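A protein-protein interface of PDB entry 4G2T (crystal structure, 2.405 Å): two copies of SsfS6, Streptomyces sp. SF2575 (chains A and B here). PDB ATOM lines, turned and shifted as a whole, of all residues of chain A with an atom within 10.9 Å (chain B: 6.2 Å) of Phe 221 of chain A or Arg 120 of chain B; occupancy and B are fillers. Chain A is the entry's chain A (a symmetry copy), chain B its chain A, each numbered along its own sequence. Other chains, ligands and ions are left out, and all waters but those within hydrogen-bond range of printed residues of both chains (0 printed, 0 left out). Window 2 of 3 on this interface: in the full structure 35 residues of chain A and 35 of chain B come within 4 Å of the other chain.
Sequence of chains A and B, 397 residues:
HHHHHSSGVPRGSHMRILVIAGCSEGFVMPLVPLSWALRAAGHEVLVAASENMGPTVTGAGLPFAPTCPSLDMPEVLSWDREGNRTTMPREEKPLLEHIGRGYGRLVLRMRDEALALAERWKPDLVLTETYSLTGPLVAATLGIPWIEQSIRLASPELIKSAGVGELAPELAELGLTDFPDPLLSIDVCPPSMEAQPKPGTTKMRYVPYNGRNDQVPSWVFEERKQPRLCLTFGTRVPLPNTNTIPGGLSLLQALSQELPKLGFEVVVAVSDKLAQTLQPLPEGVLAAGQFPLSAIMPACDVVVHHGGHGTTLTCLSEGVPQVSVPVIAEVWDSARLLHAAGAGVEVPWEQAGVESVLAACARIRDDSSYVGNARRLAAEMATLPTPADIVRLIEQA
The backbone carbonyl oxygen (O) of Phe 64 of chain B sits at hydrogen-bond distance from the backbone NH (N) of Val 216 of chain A (2.9 Å).
O of Gln 215 of chain A lies within hydrogen-bond range of ND2 of Asn 213 of chain A, 3.0 Å away. O of Trp 121 of chain B lies within hydrogen-bond range of NH1 of Arg 16 of chain B, 3.3 Å away.
Among the printed residues, pairs that only touch across the chains: Asp 214 of chain A with Phe 64 of chain B (3.6 Å), Gln 215 of chain A with Phe 64 of chain B (3.4 Å), Val 216 of chain A with Leu 46 of chain B (3.9 Å), Phe 221 of chain A with Leu 46 of chain B (3.9 Å), Phe 221 of chain A with Leu 117 of chain B (3.7 Å), Phe 221 of chain A with Arg 120 of chain B (3.7 Å), Phe 221 of chain A with Trp 121 of chain B (3.6 Å) and Glu 222 of chain A with Arg 120 of chain B (3.8 Å).
Phe 221 of chain A touches just these residues of chain B: Leu 46 (3.9 Å), Leu 117 (3.7 Å), Arg 120 (3.7 Å) and Trp 121 (3.6 Å). Arg 120 of chain B touches just these residues of chain A: Phe 221 and Glu 222. Ala 116 of chain B touches none of the printed residues of chain A. Leu 117 of chain B touches one residue of chain A. No residue of chain A comes within 4 Å of Ala 118 of chain B. No residue of chain A comes within 4 Å of Glu 119 of chain B. No residue of chain A comes within 4 Å of Lys 122 of chain B. Of the printed residues of chain B, Val 216 of chain A touches Leu 46 and Phe 64. Printed residues of chain A within 4 Å of Leu 46 of chain B: Val 216 (3.9 Å) and Phe 221 (3.9 Å). Of the printed residues of chain A, Phe 64 of chain B touches Asp 214, Gln 215 and Val 216. Of the printed residues of chain B, Asp 214 of chain A touches Phe 64. Of the printed residues of chain B, Glu 222 of chain A touches Arg 120 (3.8 Å). The nearest residue of chain A that does not touch Arg 120 of chain B is Ser 218 of chain A (6.0 Å). The nearest printed residue of chain A that does not touch Phe 64 of chain B is Phe 221 of chain A (5.7 Å).
Of the 24 printed residues of chain A, 5 touch a printed residue of chain B. Printed residues of chain A that touch a printed residue of chain B: Asp 214, Gln 215, Val 216, Phe 221 and Glu 222. Hydrophobic or aromatic side chains of chain B that line the printed part of chain A: Leu 46, Phe 64, Leu 117 and Trp 121. Among the printed residues, no Asp or Glu carboxylate lies within 4 Å of a Lys or Arg side-chain nitrogen of the other chain.
No position is printed for both chains. Of the 9 pairs that touch across the chains among the printed residues, none has its exchanged pair printed and touching as well.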
ATOM      1  N   ASN A 213      29.046  20.277  -7.121  1.00  0.00           N
ATOM      2  CA  ASN A 213      28.092  20.602  -6.066  1.00  0.00           C
ATOM      3  C   ASN A 213      26.918  19.633  -6.111  1.00  0.00           C
ATOM      4  O   ASN A 213      26.748  18.921  -7.093  1.00  0.00           O
ATOM      5  CB  ASN A 213      27.591  22.036  -6.226  1.00  0.00           C
ATOM      6  CG  ASN A 213      26.933  22.568  -4.970  1.00  0.00           C
ATOM      7  OD1 ASN A 213      27.153  22.055  -3.874  1.00  0.00           O
ATOM      8  ND2 ASN A 213      26.120  23.606  -5.124  1.00  0.00           N
ATOM      9  N   ASP A 214      26.113  19.605  -5.053  1.00  0.00           N
ATOM     10  CA  ASP A 214      24.952  18.719  -5.005  1.00  0.00           C
ATOM     11  C   ASP A 214      23.920  19.088  -6.069  1.00  0.00           C
ATOM     12  O   ASP A 214      23.341  18.214  -6.715  1.00  0.00           O
ATOM     13  CB  ASP A 214      24.311  18.742  -3.616  1.00  0.00           C
ATOM     14  CG  ASP A 214      25.215  18.159  -2.548  1.00  0.00           C
ATOM     15  OD1 ASP A 214      26.047  17.288  -2.882  1.00  0.00           O
ATOM     16  OD2 ASP A 214      25.094  18.570  -1.375  1.00  0.00           O
ATOM     17  N   GLN A 215      23.703  20.388  -6.243  1.00  0.00           N
ATOM     18  CA  GLN A 215      22.791  20.894  -7.263  1.00  0.00           C
ATOM     19  C   GLN A 215      22.983  22.389  -7.453  1.00  0.00           C
ATOM     20  O   GLN A 215      23.601  23.057  -6.625  1.00  0.00           O
ATOM     21  CB  GLN A 215      21.335  20.624  -6.878  1.00  0.00           C
ATOM     22  CG  GLN A 215      20.891  21.337  -5.611  1.00  0.00           C
ATOM     23  CD  GLN A 215      19.384  21.470  -5.510  1.00  0.00           C
ATOM     24  OE1 GLN A 215      18.776  21.055  -4.523  1.00  0.00           O
ATOM     25  NE2 GLN A 215      18.774  22.062  -6.529  1.00  0.00           N
ATOM     26  N   VAL A 216      22.451  22.911  -8.552  1.00  0.00           N
ATOM     27  CA  VAL A 216      22.416  24.348  -8.766  1.00  0.00           C
ATOM     28  C   VAL A 216      21.453  24.952  -7.753  1.00  0.00           C
ATOM     29  O   VAL A 216      20.298  24.536  -7.674  1.00  0.00           O
ATOM     30  CB  VAL A 216      21.942  24.696 -10.187  1.00  0.00           C
ATOM     31  CG1 VAL A 216      21.951  26.204 -10.393  1.00  0.00           C
ATOM     32  CG2 VAL A 216      22.818  24.006 -11.221  1.00  0.00           C
ATOM     33  N   PRO A 217      21.938  25.925  -6.963  1.00  0.00           N
ATOM     34  CA  PRO A 217      21.149  26.590  -5.920  1.00  0.00           C
ATOM     35  C   PRO A 217      19.809  27.095  -6.442  1.00  0.00           C
ATOM     36  O   PRO A 217      19.724  27.580  -7.569  1.00  0.00           O
ATOM     37  CB  PRO A 217      22.042  27.761  -5.511  1.00  0.00           C
ATOM     38  CG  PRO A 217      23.422  27.274  -5.773  1.00  0.00           C
ATOM     39  CD  PRO A 217      23.319  26.434  -7.014  1.00  0.00           C
ATOM     40  N   SER A 218      18.774  26.967  -5.618  1.00  0.00           N
ATOM     41  CA  SER A 218      17.413  27.310  -6.012  1.00  0.00           C
ATOM     42  C   SER A 218      17.244  28.792  -6.345  1.00  0.00           C
ATOM     43  O   SER A 218      16.429  29.155  -7.194  1.00  0.00           O
ATOM     44  CB  SER A 218      16.432  26.901  -4.911  1.00  0.00           C
ATOM     45  OG  SER A 218      15.119  27.343  -5.202  1.00  0.00           O
ATOM     46  N   TRP A 219      18.017  29.643  -5.678  1.00  0.00           N
ATOM     47  CA  TRP A 219      17.902  31.087  -5.869  1.00  0.00           C
ATOM     48  C   TRP A 219      18.475  31.569  -7.202  1.00  0.00           C
ATOM     49  O   TRP A 219      18.269  32.714  -7.594  1.00  0.00           O
ATOM     50  CB  TRP A 219      18.546  31.843  -4.703  1.00  0.00           C
ATOM     51  CG  TRP A 219      19.915  31.354  -4.327  1.00  0.00           C
ATOM     52  CD1 TRP A 219      20.226  30.488  -3.319  1.00  0.00           C
ATOM     53  CD2 TRP A 219      21.158  31.710  -4.945  1.00  0.00           C
ATOM     54  NE1 TRP A 219      21.583  30.280  -3.272  1.00  0.00           N
ATOM     55  CE2 TRP A 219      22.179  31.019  -4.262  1.00  0.00           C
ATOM     56  CE3 TRP A 219      21.507  32.546  -6.012  1.00  0.00           C
ATOM     57  CZ2 TRP A 219      23.523  31.135  -4.610  1.00  0.00           C
ATOM     58  CZ3 TRP A 219      22.842  32.660  -6.356  1.00  0.00           C
ATOM     59  CH2 TRP A 219      23.834  31.959  -5.658  1.00  0.00           C
ATOM     60  N   VAL A 220      19.191  30.690  -7.896  1.00  0.00           N
ATOM     61  CA  VAL A 220      19.769  31.028  -9.193  1.00  0.00           C
ATOM     62  C   VAL A 220      18.682  31.213 -10.253  1.00  0.00           C
ATOM     63  O   VAL A 220      18.778  32.092 -11.110  1.00  0.00           O
ATOM     64  CB  VAL A 220      20.770  29.948  -9.663  1.00  0.00           C
ATOM     65  CG1 VAL A 220      21.328  30.288 -11.037  1.00  0.00           C
ATOM     66  CG2 VAL A 220      21.897  29.796  -8.654  1.00  0.00           C
ATOM     67  N   PHE A 221      17.641  30.390 -10.175  1.00  0.00           N
ATOM     68  CA  PHE A 221      16.588  30.393 -11.187  1.00  0.00           C
ATOM     69  C   PHE A 221      15.513  31.451 -10.937  1.00  0.00           C
ATOM     70  O   PHE A 221      14.988  32.044 -11.879  1.00  0.00           O
ATOM     71  CB  PHE A 221      15.947  29.007 -11.293  1.00  0.00           C
ATOM     72  CG  PHE A 221      16.934  27.903 -11.545  1.00  0.00           C
ATOM     73  CD1 PHE A 221      17.569  27.791 -12.771  1.00  0.00           C
ATOM     74  CD2 PHE A 221      17.224  26.977 -10.558  1.00  0.00           C
ATOM     75  CE1 PHE A 221      18.479  26.777 -13.006  1.00  0.00           C
ATOM     76  CE2 PHE A 221      18.133  25.960 -10.787  1.00  0.00           C
ATOM     77  CZ  PHE A 221      18.761  25.859 -12.012  1.00  0.00           C
ATOM     78  N   GLU A 222      15.187  31.682  -9.669  1.00  0.00           N
ATOM     79  CA  GLU A 222      14.171  32.666  -9.314  1.00  0.00           C
ATOM     80  C   GLU A 222      14.653  34.093  -9.560  1.00  0.00           C
ATOM     81  O   GLU A 222      15.850  34.338  -9.710  1.00  0.00           O
ATOM     82  CB  GLU A 222      13.726  32.483  -7.863  1.00  0.00           C
ATOM     83  CG  GLU A 222      12.806  31.290  -7.657  1.00  0.00           C
ATOM     84  CD  GLU A 222      12.660  30.905  -6.199  1.00  0.00           C
ATOM     85  OE1 GLU A 222      13.659  30.997  -5.457  1.00  0.00           O
ATOM     86  OE2 GLU A 222      11.545  30.511  -5.796  1.00  0.00           O
ATOM     87  N   GLU A 223      13.714  35.032  -9.600  1.00  0.00           N
ATOM     88  CA  GLU A 223      14.026  36.417  -9.933  1.00  0.00           C
ATOM     89  C   GLU A 223      14.828  37.121  -8.841  1.00  0.00           C
ATOM     90  O   GLU A 223      14.748  36.766  -7.666  1.00  0.00           O
ATOM     91  CB  GLU A 223      12.748  37.197 -10.251  1.00  0.00           C
ATOM     92  CG  GLU A 223      11.930  36.586 -11.375  1.00  0.00           C
ATOM     93  CD  GLU A 223      11.273  37.630 -12.255  1.00  0.00           C
ATOM     94  OE1 GLU A 223      10.396  38.368 -11.756  1.00  0.00           O
ATOM     95  OE2 GLU A 223      11.638  37.715 -13.446  1.00  0.00           O
ATOM     96  N   ARG A 224      15.599  38.123  -9.248  1.00  0.00           N
ATOM     97  CA  ARG A 224      16.481  38.846  -8.341  1.00  0.00           C
ATOM     98  C   ARG A 224      16.057  40.308  -8.222  1.00  0.00           C
ATOM     99  O   ARG A 224      16.110  41.056  -9.198  1.00  0.00           O
ATOM    100  CB  ARG A 224      17.925  38.751  -8.840  1.00  0.00           C
ATOM    101  CG  ARG A 224      18.935  39.476  -7.976  1.00  0.00           C
ATOM    102  CD  ARG A 224      20.366  39.120  -8.357  1.00  0.00           C
ATOM    103  NE  ARG A 224      20.784  39.701  -9.632  1.00  0.00           N
ATOM    104  CZ  ARG A 224      20.812  39.038 -10.784  1.00  0.00           C
ATOM    105  NH1 ARG A 224      20.444  37.765 -10.829  1.00  0.00           N
ATOM    106  NH2 ARG A 224      21.211  39.648 -11.891  1.00  0.00           N
ATOM    107  N   LYS A 225      15.639  40.713  -7.025  1.00  0.00           N
ATOM    108  CA  LYS A 225      15.127  42.067  -6.822  1.00  0.00           C
ATOM    109  C   LYS A 225      16.110  43.011  -6.126  1.00  0.00           C
ATOM    110  O   LYS A 225      15.715  44.062  -5.618  1.00  0.00           O
ATOM    111  CB  LYS A 225      13.784  42.045  -6.079  1.00  0.00           C
ATOM    112  CG  LYS A 225      13.814  41.377  -4.712  1.00  0.00           C
ATOM    113  CD  LYS A 225      12.498  41.602  -3.977  1.00  0.00           C
ATOM    114  CE  LYS A 225      12.456  40.859  -2.652  1.00  0.00           C
ATOM    115  NZ  LYS A 225      12.381  39.384  -2.840  1.00  0.00           N
ATOM    116  N   ARG A 228      23.163  41.295  -6.504  1.00  0.00           N
ATOM    117  CA  ARG A 228      23.777  40.204  -5.756  1.00  0.00           C
ATOM    118  C   ARG A 228      25.286  40.149  -5.978  1.00  0.00           C
ATOM    119  O   ARG A 228      25.760  40.236  -7.111  1.00  0.00           O
ATOM    120  CB  ARG A 228      23.128  38.864  -6.120  1.00  0.00           C
ATOM    121  CG  ARG A 228      23.589  37.695  -5.262  1.00  0.00           C
ATOM    122  CD  ARG A 228      22.832  36.411  -5.586  1.00  0.00           C
ATOM    123  NE  ARG A 228      21.419  36.484  -5.219  1.00  0.00           N
ATOM    124  CZ  ARG A 228      20.415  36.264  -6.063  1.00  0.00           C
ATOM    125  NH1 ARG A 228      20.664  35.953  -7.327  1.00  0.00           N
ATOM    126  NH2 ARG A 228      19.162  36.351  -5.641  1.00  0.00           N
ATOM    127  N   GLU A 265      23.093  41.915  -1.856  1.00  0.00           N
ATOM    128  CA  GLU A 265      22.817  40.595  -1.312  1.00  0.00           C
ATOM    129  C   GLU A 265      24.041  39.752  -1.624  1.00  0.00           C
ATOM    130  O   GLU A 265      24.388  39.573  -2.788  1.00  0.00           O
ATOM    131  CB  GLU A 265      21.578  39.991  -1.970  1.00  0.00           C
ATOM    132  CG  GLU A 265      21.230  38.596  -1.480  1.00  0.00           C
ATOM    133  CD  GLU A 265      20.096  37.969  -2.267  1.00  0.00           C
ATOM    134  OE1 GLU A 265      19.902  38.352  -3.440  1.00  0.00           O
ATOM    135  OE2 GLU A 265      19.396  37.096  -1.713  1.00  0.00           O
ATOM    136  N   LEU A 286      23.163  35.723   1.555  1.00  0.00           N
ATOM    137  CA  LEU A 286      22.135  34.815   1.085  1.00  0.00           C
ATOM    138  C   LEU A 286      22.515  33.394   1.469  1.00  0.00           C
ATOM    139  O   LEU A 286      21.704  32.649   2.018  1.00  0.00           O
ATOM    140  CB  LEU A 286      21.966  34.941  -0.425  1.00  0.00           C
ATOM    141  CG  LEU A 286      20.974  33.974  -1.065  1.00  0.00           C
ATOM    142  CD1 LEU A 286      19.607  34.086  -0.404  1.00  0.00           C
ATOM    143  CD2 LEU A 286      20.876  34.241  -2.555  1.00  0.00           C
ATOM    144  N   PRO A 292      30.099  26.084  -7.366  1.00  0.00           N
ATOM    145  CA  PRO A 292      30.782  26.237  -8.652  1.00  0.00           C
ATOM    146  C   PRO A 292      30.333  27.538  -9.300  1.00  0.00           C
ATOM    147  O   PRO A 292      29.139  27.715  -9.543  1.00  0.00           O
ATOM    148  CB  PRO A 292      30.277  25.038  -9.456  1.00  0.00           C
ATOM    149  CG  PRO A 292      29.969  24.011  -8.423  1.00  0.00           C
ATOM    150  CD  PRO A 292      29.430  24.779  -7.250  1.00  0.00           C
ATOM    151  N   SER A 294      30.380  29.007 -12.220  1.00  0.00           N
ATOM    152  CA  SER A 294      29.619  28.980 -13.469  1.00  0.00           C
ATOM    153  C   SER A 294      28.131  28.713 -13.241  1.00  0.00           C
ATOM    154  O   SER A 294      27.291  29.108 -14.048  1.00  0.00           O
ATOM    155  CB  SER A 294      30.192  27.935 -14.428  1.00  0.00           C
ATOM    156  OG  SER A 294      30.164  26.642 -13.850  1.00  0.00           O
ATOM    157  N   ALA A 295      27.814  28.043 -12.137  1.00  0.00           N
ATOM    158  CA  ALA A 295      26.432  27.735 -11.802  1.00  0.00           C
ATOM    159  C   ALA A 295      25.708  28.932 -11.188  1.00  0.00           C
ATOM    160  O   ALA A 295      24.497  29.080 -11.349  1.00  0.00           O
ATOM    161  CB  ALA A 295      26.369  26.536 -10.863  1.00  0.00           C
ATOM    162  N   ILE A 296      26.450  29.787 -10.489  1.00  0.00           N
ATOM    163  CA  ILE A 296      25.842  30.910  -9.776  1.00  0.00           C
ATOM    164  C   ILE A 296      26.085  32.268 -10.437  1.00  0.00           C
ATOM    165  O   ILE A 296      25.416  33.246 -10.106  1.00  0.00           O
ATOM    166  CB  ILE A 296      26.319  30.979  -8.309  1.00  0.00           C
ATOM    167  CG1 ILE A 296      27.815  31.291  -8.244  1.00  0.00           C
ATOM    168  CG2 ILE A 296      26.000  29.682  -7.581  1.00  0.00           C
ATOM    169  CD1 ILE A 296      28.332  31.508  -6.838  1.00  0.00           C
ATOM    170  N   MET A 297      27.040  32.324 -11.362  1.00  0.00           N
ATOM    171  CA  MET A 297      27.372  33.571 -12.063  1.00  0.00           C
ATOM    172  C   MET A 297      26.202  34.307 -12.736  1.00  0.00           C
ATOM    173  O   MET A 297      26.123  35.532 -12.644  1.00  0.00           O
ATOM    174  CB  MET A 297      28.520  33.364 -13.062  1.00  0.00           C
ATOM    175  CG  MET A 297      29.915  33.393 -12.446  1.00  0.00           C
ATOM    176  SD  MET A 297      30.295  35.013 -11.426  1.00  0.00           S
ATOM    177  CE  MET A 297      29.852  34.373  -9.634  1.00  0.00           C
ATOM    178  N   PRO A 298      25.298  33.579 -13.424  1.00  0.00           N
ATOM    179  CA  PRO A 298      24.152  34.288 -14.011  1.00  0.00           C
ATOM    180  C   PRO A 298      23.276  34.990 -12.973  1.00  0.00           C
ATOM    181  O   PRO A 298      22.553  35.923 -13.316  1.00  0.00           O
ATOM    182  CB  PRO A 298      23.359  33.166 -14.686  1.00  0.00           C
ATOM    183  CG  PRO A 298      24.375  32.138 -15.009  1.00  0.00           C
ATOM    184  CD  PRO A 298      25.347  32.173 -13.869  1.00  0.00           C
ATOM    185  N   ALA A 299      23.347  34.545 -11.723  1.00  0.00           N
ATOM    186  CA  ALA A 299      22.539  35.127 -10.658  1.00  0.00           C
ATOM    187  C   ALA A 299      23.295  36.206  -9.884  1.00  0.00           C
ATOM    188  O   ALA A 299      22.833  36.665  -8.840  1.00  0.00           O
ATOM    189  CB  ALA A 299      22.051  34.038  -9.712  1.00  0.00           C
ATOM    190  N   CYS A 300      24.450  36.610 -10.401  1.00  0.00           N
ATOM    191  CA  CYS A 300      25.280  37.607  -9.728  1.00  0.00           C
ATOM    192  C   CYS A 300      25.538  38.834 -10.600  1.00  0.00           C
ATOM    193  O   CYS A 300      25.414  38.777 -11.824  1.00  0.00           O
ATOM    194  CB  CYS A 300      26.609  36.989  -9.289  1.00  0.00           C
ATOM    195  SG  CYS A 300      26.452  35.665  -8.068  1.00  0.00           S
ATOM    196  N   ARG B  16      21.339  27.073 -24.690  1.00  0.00           N
ATOM    197  CA  ARG B  16      21.040  26.531 -23.373  1.00  0.00           C
ATOM    198  C   ARG B  16      20.254  25.237 -23.549  1.00  0.00           C
ATOM    199  O   ARG B  16      19.111  25.254 -24.005  1.00  0.00           O
ATOM    200  CB  ARG B  16      20.241  27.535 -22.541  1.00  0.00           C
ATOM    201  CG  ARG B  16      21.011  28.098 -21.359  1.00  0.00           C
ATOM    202  CD  ARG B  16      20.257  29.222 -20.669  1.00  0.00           C
ATOM    203  NE  ARG B  16      20.950  29.673 -19.465  1.00  0.00           N
ATOM    204  CZ  ARG B  16      20.603  30.743 -18.758  1.00  0.00           C
ATOM    205  NH1 ARG B  16      19.570  31.484 -19.135  1.00  0.00           N
ATOM    206  NH2 ARG B  16      21.293  31.076 -17.675  1.00  0.00           N
ATOM    207  N   LEU B  46      22.224  21.775 -18.532  1.00  0.00           N
ATOM    208  CA  LEU B  46      21.672  21.532 -17.206  1.00  0.00           C
ATOM    209  C   LEU B  46      20.903  20.219 -17.210  1.00  0.00           C
ATOM    210  O   LEU B  46      19.939  20.056 -17.958  1.00  0.00           O
ATOM    211  CB  LEU B  46      20.752  22.676 -16.782  1.00  0.00           C
ATOM    212  CG  LEU B  46      20.056  22.497 -15.430  1.00  0.00           C
ATOM    213  CD1 LEU B  46      21.078  22.390 -14.307  1.00  0.00           C
ATOM    214  CD2 LEU B  46      19.079  23.633 -15.166  1.00  0.00           C
ATOM    215  N   PHE B  64      23.194  20.052 -11.922  1.00  0.00           N
ATOM    216  CA  PHE B  64      22.004  19.253 -11.646  1.00  0.00           C
ATOM    217  C   PHE B  64      20.855  20.050 -11.034  1.00  0.00           C
ATOM    218  O   PHE B  64      21.068  20.969 -10.245  1.00  0.00           O
ATOM    219  CB  PHE B  64      22.353  18.072 -10.736  1.00  0.00           C
ATOM    220  CG  PHE B  64      21.154  17.307 -10.246  1.00  0.00           C
ATOM    221  CD1 PHE B  64      20.501  16.412 -11.076  1.00  0.00           C
ATOM    222  CD2 PHE B  64      20.683  17.484  -8.954  1.00  0.00           C
ATOM    223  CE1 PHE B  64      19.397  15.710 -10.629  1.00  0.00           C
ATOM    224  CE2 PHE B  64      19.580  16.784  -8.501  1.00  0.00           C
ATOM    225  CZ  PHE B  64      18.937  15.895  -9.340  1.00  0.00           C
ATOM    226  N   ALA B  65      19.635  19.677 -11.408  1.00  0.00           N
ATOM    227  CA  ALA B  65      18.428  20.239 -10.816  1.00  0.00           C
ATOM    228  C   ALA B  65      17.367  19.148 -10.687  1.00  0.00           C
ATOM    229  O   ALA B  65      17.052  18.469 -11.664  1.00  0.00           O
ATOM    230  CB  ALA B  65      17.912  21.390 -11.657  1.00  0.00           C
ATOM    231  N   LEU B 115       8.881  21.559 -15.785  1.00  0.00           N
ATOM    232  CA  LEU B 115       8.318  22.651 -16.569  1.00  0.00           C
ATOM    233  C   LEU B 115       8.702  23.989 -15.953  1.00  0.00           C
ATOM    234  O   LEU B 115       9.206  24.872 -16.642  1.00  0.00           O
ATOM    235  CB  LEU B 115       6.796  22.530 -16.658  1.00  0.00           C
ATOM    236  CG  LEU B 115       6.139  23.233 -17.845  1.00  0.00           C
ATOM    237  CD1 LEU B 115       6.692  22.682 -19.149  1.00  0.00           C
ATOM    238  CD2 LEU B 115       4.627  23.078 -17.793  1.00  0.00           C
ATOM    239  N   ALA B 116       8.467  24.124 -14.651  1.00  0.00           N
ATOM    240  CA  ALA B 116       8.792  25.346 -13.921  1.00  0.00           C
ATOM    241  C   ALA B 116      10.275  25.683 -14.030  1.00  0.00           C
ATOM    242  O   ALA B 116      10.652  26.852 -14.119  1.00  0.00           O
ATOM    243  CB  ALA B 116       8.383  25.214 -12.461  1.00  0.00           C
ATOM    244  N   LEU B 117      11.113  24.651 -14.026  1.00  0.00           N
ATOM    245  CA  LEU B 117      12.547  24.825 -14.214  1.00  0.00           C
ATOM    246  C   LEU B 117      12.836  25.288 -15.636  1.00  0.00           C
ATOM    247  O   LEU B 117      13.767  26.057 -15.872  1.00  0.00           O
ATOM    248  CB  LEU B 117      13.283  23.515 -13.927  1.00  0.00           C
ATOM    249  CG  LEU B 117      14.793  23.471 -14.168  1.00  0.00           C
ATOM    250  CD1 LEU B 117      15.530  24.352 -13.169  1.00  0.00           C
ATOM    251  CD2 LEU B 117      15.293  22.036 -14.105  1.00  0.00           C
ATOM    252  N   ALA B 118      12.029  24.818 -16.582  1.00  0.00           N
ATOM    253  CA  ALA B 118      12.195  25.183 -17.984  1.00  0.00           C
ATOM    254  C   ALA B 118      11.710  26.605 -18.258  1.00  0.00           C
ATOM    255  O   ALA B 118      12.230  27.286 -19.140  1.00  0.00           O
ATOM    256  CB  ALA B 118      11.473  24.189 -18.883  1.00  0.00           C
ATOM    257  N   GLU B 119      10.708  27.046 -17.502  1.00  0.00           N
ATOM    258  CA  GLU B 119      10.189  28.403 -17.632  1.00  0.00           C
ATOM    259  C   GLU B 119      11.248  29.417 -17.220  1.00  0.00           C
ATOM    260  O   GLU B 119      11.454  30.429 -17.889  1.00  0.00           O
ATOM    261  CB  GLU B 119       8.946  28.590 -16.757  1.00  0.00           C
ATOM    262  CG  GLU B 119       7.815  27.607 -17.017  1.00  0.00           C
ATOM    263  CD  GLU B 119       6.808  28.114 -18.030  1.00  0.00           C
ATOM    264  OE1 GLU B 119       5.595  27.915 -17.806  1.00  0.00           O
ATOM    265  OE2 GLU B 119       7.224  28.704 -19.048  1.00  0.00           O
ATOM    266  N   ARG B 120      11.922  29.129 -16.111  1.00  0.00           N
ATOM    267  CA  ARG B 120      12.877  30.060 -15.519  1.00  0.00           C
ATOM    268  C   ARG B 120      14.255  30.013 -16.176  1.00  0.00           C
ATOM    269  O   ARG B 120      14.887  31.050 -16.374  1.00  0.00           O
ATOM    270  CB  ARG B 120      12.991  29.810 -14.013  1.00  0.00           C
ATOM    271  CG  ARG B 120      11.725  30.159 -13.247  1.00  0.00           C
ATOM    272  CD  ARG B 120      11.730  29.586 -11.840  1.00  0.00           C
ATOM    273  NE  ARG B 120      10.558  30.023 -11.085  1.00  0.00           N
ATOM    274  CZ  ARG B 120      10.181  29.508  -9.920  1.00  0.00           C
ATOM    275  NH1 ARG B 120      10.879  28.526  -9.367  1.00  0.00           N
ATOM    276  NH2 ARG B 120       9.100  29.974  -9.308  1.00  0.00           N
ATOM    277  N   TRP B 121      14.718  28.814 -16.514  1.00  0.00           N
ATOM    278  CA  TRP B 121      16.043  28.658 -17.108  1.00  0.00           C
ATOM    279  C   TRP B 121      16.029  28.985 -18.599  1.00  0.00           C
ATOM    280  O   TRP B 121      17.050  29.384 -19.162  1.00  0.00           O
ATOM    281  CB  TRP B 121      16.581  27.244 -16.872  1.00  0.00           C
ATOM    282  CG  TRP B 121      18.065  27.128 -17.064  1.00  0.00           C
ATOM    283  CD1 TRP B 121      19.033  27.790 -16.367  1.00  0.00           C
ATOM    284  CD2 TRP B 121      18.748  26.290 -18.005  1.00  0.00           C
ATOM    285  NE1 TRP B 121      20.277  27.423 -16.820  1.00  0.00           N
ATOM    286  CE2 TRP B 121      20.131  26.503 -17.823  1.00  0.00           C
ATOM    287  CE3 TRP B 121      18.328  25.384 -18.982  1.00  0.00           C
ATOM    288  CZ2 TRP B 121      21.093  25.842 -18.585  1.00  0.00           C
ATOM    289  CZ3 TRP B 121      19.285  24.729 -19.736  1.00  0.00           C
ATOM    290  CH2 TRP B 121      20.651  24.962 -19.534  1.00  0.00           C
ATOM    291  N   LYS B 122      14.866  28.811 -19.223  1.00  0.00           N
ATOM    292  CA  LYS B 122      14.665  29.125 -20.639  1.00  0.00           C
ATOM    293  C   LYS B 122      15.666  28.443 -21.568  1.00  0.00           C
ATOM    294  O   LYS B 122      16.585  29.086 -22.075  1.00  0.00           O
ATOM    295  CB  LYS B 122      14.693  30.640 -20.864  1.00  0.00           C
ATOM    296  CG  LYS B 122      13.574  31.390 -20.163  1.00  0.00           C
ATOM    297  CD  LYS B 122      13.768  32.893 -20.267  1.00  0.00           C
ATOM    298  CE  LYS B 122      12.579  33.643 -19.688  1.00  0.00           C
ATOM    299  NZ  LYS B 122      12.320  33.273 -18.269  1.00  0.00           N
